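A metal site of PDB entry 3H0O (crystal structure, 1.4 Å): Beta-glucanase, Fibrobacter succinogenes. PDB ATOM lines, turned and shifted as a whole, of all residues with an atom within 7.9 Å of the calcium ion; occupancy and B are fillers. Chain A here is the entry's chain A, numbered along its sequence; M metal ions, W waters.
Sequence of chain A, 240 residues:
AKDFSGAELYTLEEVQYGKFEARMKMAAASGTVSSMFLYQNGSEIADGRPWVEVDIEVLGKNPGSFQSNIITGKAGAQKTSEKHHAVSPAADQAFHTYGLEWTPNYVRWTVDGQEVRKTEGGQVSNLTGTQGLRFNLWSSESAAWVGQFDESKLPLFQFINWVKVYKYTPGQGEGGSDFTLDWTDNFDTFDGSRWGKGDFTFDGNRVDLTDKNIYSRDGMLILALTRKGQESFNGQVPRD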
ATOM      1  N   ARG A  23      15.343  16.709  33.919  1.00  0.00           N
ATOM      2  CA  ARG A  23      14.745  15.395  34.212  1.00  0.00           C
ATOM      3  C   ARG A  23      15.712  14.372  33.664  1.00  0.00           C
ATOM      4  O   ARG A  23      15.845  14.227  32.453  1.00  0.00           O
ATOM      5  CB  ARG A  23      13.370  15.336  33.507  1.00  0.00           C
ATOM      6  CG  ARG A  23      12.621  14.049  33.726  1.00  0.00           C
ATOM      7  CD  ARG A  23      12.235  13.914  35.183  1.00  0.00           C
ATOM      8  NE  ARG A  23      11.408  12.721  35.397  1.00  0.00           N
ATOM      9  CZ  ARG A  23      10.948  12.353  36.585  1.00  0.00           C
ATOM     10  NH1 ARG A  23      11.211  13.083  37.655  1.00  0.00           N
ATOM     11  NH2 ARG A  23      10.255  11.211  36.702  1.00  0.00           N
ATOM     12  N   ILE A 160      18.669  12.460  29.355  1.00  0.00           N
ATOM     13  CA  ILE A 160      18.060  13.716  29.747  1.00  0.00           C
ATOM     14  C   ILE A 160      16.742  13.806  28.964  1.00  0.00           C
ATOM     15  O   ILE A 160      16.738  13.915  27.735  1.00  0.00           O
ATOM     16  CB  ILE A 160      18.961  14.916  29.400  1.00  0.00           C
ATOM     17  CG1 ILE A 160      20.377  14.718  29.972  1.00  0.00           C
ATOM     18  CG2 ILE A 160      18.325  16.185  29.954  1.00  0.00           C
ATOM     19  CD1 ILE A 160      21.334  15.875  29.647  1.00  0.00           C
ATOM     20  N   ASN A 161      15.626  13.762  29.692  1.00  0.00           N
ATOM     21  CA  ASN A 161      14.287  13.790  29.057  1.00  0.00           C
ATOM     22  C   ASN A 161      13.851  15.206  28.653  1.00  0.00           C
ATOM     23  O   ASN A 161      13.225  15.414  27.610  1.00  0.00           O
ATOM     24  CB  ASN A 161      13.296  13.167  30.048  1.00  0.00           C
ATOM     25  CG  ASN A 161      11.943  12.865  29.428  1.00  0.00           C
ATOM     26  OD1 ASN A 161      11.771  13.053  28.256  1.00  0.00           O
ATOM     27  ND2 ASN A 161      11.009  12.400  30.220  1.00  0.00           N
ATOM     28  N   TRP A 162      14.146  16.183  29.529  1.00  0.00           N
ATOM     29  CA  TRP A 162      13.781  17.572  29.262  1.00  0.00           C
ATOM     30  C   TRP A 162      14.573  18.463  30.210  1.00  0.00           C
ATOM     31  O   TRP A 162      15.089  17.999  31.244  1.00  0.00           O
ATOM     32  CB  TRP A 162      12.242  17.838  29.442  1.00  0.00           C
ATOM     33  CG  TRP A 162      11.602  17.360  30.711  1.00  0.00           C
ATOM     34  CD1 TRP A 162      10.792  16.264  30.860  1.00  0.00           C
ATOM     35  CD2 TRP A 162      11.603  18.024  31.994  1.00  0.00           C
ATOM     36  NE1 TRP A 162      10.292  16.222  32.144  1.00  0.00           N
ATOM     37  CE2 TRP A 162      10.768  17.282  32.853  1.00  0.00           C
ATOM     38  CE3 TRP A 162      12.215  19.187  32.482  1.00  0.00           C
ATOM     39  CZ2 TRP A 162      10.543  17.649  34.199  1.00  0.00           C
ATOM     40  CZ3 TRP A 162      11.995  19.556  33.836  1.00  0.00           C
ATOM     41  CH2 TRP A 162      11.166  18.787  34.656  1.00  0.00           C
ATOM     42  N   VAL A 163      14.616  19.735  29.825  1.00  0.00           N
ATOM     43  CA  VAL A 163      15.253  20.783  30.610  1.00  0.00           C
ATOM     44  C   VAL A 163      14.303  21.972  30.623  1.00  0.00           C
ATOM     45  O   VAL A 163      13.679  22.278  29.593  1.00  0.00           O
ATOM     46  CB  VAL A 163      16.607  21.239  29.961  1.00  0.00           C
ATOM     47  CG1 VAL A 163      17.017  22.655  30.419  1.00  0.00           C
ATOM     48  CG2 VAL A 163      17.697  20.223  30.355  1.00  0.00           C
ATOM     49  N   ASP A 185      13.087  22.596  26.833  1.00  0.00           N
ATOM     50  CA  ASP A 185      13.541  21.813  25.678  1.00  0.00           C
ATOM     51  C   ASP A 185      13.170  20.368  26.042  1.00  0.00           C
ATOM     52  O   ASP A 185      13.658  19.788  27.012  1.00  0.00           O
ATOM     53  CB  ASP A 185      15.043  21.918  25.449  1.00  0.00           C
ATOM     54  CG  ASP A 185      15.465  21.364  24.104  1.00  0.00           C
ATOM     55  OD1 ASP A 185      14.741  20.460  23.583  1.00  0.00           O
ATOM     56  OD2 ASP A 185      16.513  21.794  23.606  1.00  0.00           O
ATOM     57  N   ASN A 186      12.243  19.789  25.266  1.00  0.00           N
ATOM     58  CA  ASN A 186      11.809  18.423  25.482  1.00  0.00           C
ATOM     59  C   ASN A 186      12.698  17.373  24.808  1.00  0.00           C
ATOM     60  O   ASN A 186      12.429  16.191  24.902  1.00  0.00           O
ATOM     61  CB  ASN A 186      10.361  18.301  25.000  1.00  0.00           C
ATOM     62  CG  ASN A 186       9.398  18.942  25.968  1.00  0.00           C
ATOM     63  OD1 ASN A 186       9.122  18.331  26.993  1.00  0.00           O
ATOM     64  ND2 ASN A 186       8.892  20.178  25.672  1.00  0.00           N
ATOM     65  N   PHE A 187      13.738  17.831  24.141  1.00  0.00           N
ATOM     66  CA  PHE A 187      14.681  16.957  23.473  1.00  0.00           C
ATOM     67  C   PHE A 187      14.153  16.016  22.422  1.00  0.00           C
ATOM     68  O   PHE A 187      14.653  14.906  22.233  1.00  0.00           O
ATOM     69  CB  PHE A 187      15.548  16.235  24.512  1.00  0.00           C
ATOM     70  CG  PHE A 187      16.426  17.202  25.285  1.00  0.00           C
ATOM     71  CD1 PHE A 187      16.289  17.293  26.657  1.00  0.00           C
ATOM     72  CD2 PHE A 187      17.335  18.014  24.621  1.00  0.00           C
ATOM     73  CE1 PHE A 187      17.071  18.213  27.389  1.00  0.00           C
ATOM     74  CE2 PHE A 187      18.128  18.944  25.333  1.00  0.00           C
ATOM     75  CZ  PHE A 187      17.978  19.030  26.702  1.00  0.00           C
ATOM     76  N   ASP A 188      13.152  16.493  21.686  1.00  0.00           N
ATOM     77  CA  ASP A 188      12.693  15.701  20.537  1.00  0.00           C
ATOM     78  C   ASP A 188      13.788  15.739  19.482  1.00  0.00           C
ATOM     79  O   ASP A 188      13.820  14.885  18.587  1.00  0.00           O
ATOM     80  CB  ASP A 188      11.400  16.306  19.963  1.00  0.00           C
ATOM     81  CG  ASP A 188      10.176  15.915  20.758  1.00  0.00           C
ATOM     82  OD1 ASP A 188       9.110  16.559  20.536  1.00  0.00           O
ATOM     83  OD2 ASP A 188      10.222  14.979  21.592  1.00  0.00           O
ATOM     84  N   THR A 189      14.677  16.733  19.562  1.00  0.00           N
ATOM     85  CA  THR A 189      15.823  16.814  18.653  1.00  0.00           C
ATOM     86  C   THR A 189      16.915  17.486  19.443  1.00  0.00           C
ATOM     87  O   THR A 189      16.687  17.935  20.563  1.00  0.00           O
ATOM     88  CB  THR A 189      15.585  17.747  17.437  1.00  0.00           C
ATOM     89  OG1 THR A 189      15.390  19.085  17.910  1.00  0.00           O
ATOM     90  CG2 THR A 189      14.385  17.289  16.605  1.00  0.00           C
ATOM     91  N   ARG A 217      17.498  10.509  20.663  1.00  0.00           N
ATOM     92  CA  ARG A 217      16.663   9.361  20.362  1.00  0.00           C
ATOM     93  C   ARG A 217      15.416   9.317  21.227  1.00  0.00           C
ATOM     94  O   ARG A 217      15.489   9.520  22.431  1.00  0.00           O
ATOM     95  CB  ARG A 217      17.440   8.073  20.587  1.00  0.00           C
ATOM     96  CG  ARG A 217      16.870   6.875  19.854  1.00  0.00           C
ATOM     97  CD  ARG A 217      18.051   6.127  19.258  1.00  0.00           C
ATOM     98  NE  ARG A 217      18.837   7.094  18.486  1.00  0.00           N
ATOM     99  CZ  ARG A 217      20.135   6.972  18.215  1.00  0.00           C
ATOM    100  NH1 ARG A 217      20.822   5.909  18.641  1.00  0.00           N
ATOM    101  NH2 ARG A 217      20.744   7.935  17.521  1.00  0.00           N
ATOM    102  N   ASP A 218      14.287   9.055  20.585  1.00  0.00           N
ATOM    103  CA  ASP A 218      13.037   8.870  21.277  1.00  0.00           C
ATOM    104  C   ASP A 218      12.708   9.874  22.352  1.00  0.00           C
ATOM    105  O   ASP A 218      12.346   9.487  23.462  1.00  0.00           O
ATOM    106  CB  ASP A 218      12.991   7.474  21.904  1.00  0.00           C
ATOM    107  CG  ASP A 218      13.040   6.384  20.859  1.00  0.00           C
ATOM    108  OD1 ASP A 218      13.200   5.206  21.262  1.00  0.00           O
ATOM    109  OD2 ASP A 218      12.896   6.700  19.654  1.00  0.00           O
ATOM    110  N   GLY A 219      12.882  11.151  22.016  1.00  0.00           N
ATOM    111  CA  GLY A 219      12.529  12.197  22.961  1.00  0.00           C
ATOM    112  C   GLY A 219      13.534  12.489  24.052  1.00  0.00           C
ATOM    113  O   GLY A 219      13.211  13.221  24.971  1.00  0.00           O
ATOM    114  N   MET A 220      14.701  11.861  23.984  1.00  0.00           N
ATOM    115  CA  MET A 220      15.728  12.121  24.982  1.00  0.00           C
ATOM    116  C   MET A 220      17.063  12.455  24.384  1.00  0.00           C
ATOM    117  O   MET A 220      17.387  12.107  23.263  1.00  0.00           O
ATOM    118  CB  MET A 220      15.892  10.924  25.880  1.00  0.00           C
ATOM    119  CG  MET A 220      14.592  10.550  26.545  1.00  0.00           C
ATOM    120  SD  MET A 220      14.846  10.113  28.216  1.00  0.00           S
ATOM    121  CE  MET A 220      13.187   9.402  28.614  1.00  0.00           C
ATOM    122  N   LEU A 221      17.855  13.192  25.138  1.00  0.00           N
ATOM    123  CA  LEU A 221      19.210  13.472  24.724  1.00  0.00           C
ATOM    124  C   LEU A 221      20.008  12.455  25.547  1.00  0.00           C
ATOM    125  O   LEU A 221      19.778  12.292  26.736  1.00  0.00           O
ATOM    126  CB  LEU A 221      19.574  14.881  25.160  1.00  0.00           C
ATOM    127  CG  LEU A 221      20.821  15.633  24.664  1.00  0.00           C
ATOM    128  CD1 LEU A 221      22.088  15.071  25.330  1.00  0.00           C
ATOM    129  CD2 LEU A 221      20.848  15.633  23.105  1.00  0.00           C
ATOM    130  N   ASP A 240       9.966   7.269  30.773  1.00  0.00           N
ATOM    131  CA  ASP A 240       9.901   8.069  31.984  1.00  0.00           C
ATOM    132  C   ASP A 240       8.452   8.316  32.418  1.00  0.00           C
ATOM    133  O   ASP A 240       7.690   8.936  31.677  1.00  0.00           O
ATOM    134  CB  ASP A 240      10.652   9.372  31.794  1.00  0.00           C
ATOM    135  CG  ASP A 240      10.605  10.244  33.018  1.00  0.00           C
ATOM    136  OD1 ASP A 240      10.894  11.446  32.884  1.00  0.00           O
ATOM    137  OD2 ASP A 240      10.261   9.723  34.118  1.00  0.00           O
HETATM  138 CA    CA M   1      11.617  14.324  26.204  1.00  0.00          CA
HETATM  139  O   HOH W   1       9.873  15.551  27.376  1.00  0.00           O
HETATM  140  O   HOH W   2      10.116  14.652  24.308  1.00  0.00           O
HETATM  141  O   HOH W   3      10.189  12.461  26.107  1.00  0.00           O
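The backbone NH (N) of Asn 161 sits at hydrogen-bond distance from the backbone carbonyl oxygen (O) of Arg 23 (2.8 Å). The side-chain amide nitrogen of Asn 161 lies within hydrogen-bond range of the side-chain carboxylate of Asp 240 (2.8 Å).
The calcium ion is bound by O of Gly 219 (2.3 Å). The calcium ion is bound by water W3 (2.3 Å). The backbone carbonyl oxygen (O) of Asn 161 is bound to the calcium ion, 2.4 Å away. The calcium ion is bound by O of Asn 186 (2.4 Å). The calcium ion is bound by OD1 of Asn 161 (2.4 Å). The calcium ion is bound by water W1, at 2.4 Å. The calcium ion is bound by water W2, at 2.4 Å. The calcium ion has seven donor atoms within binding distance.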
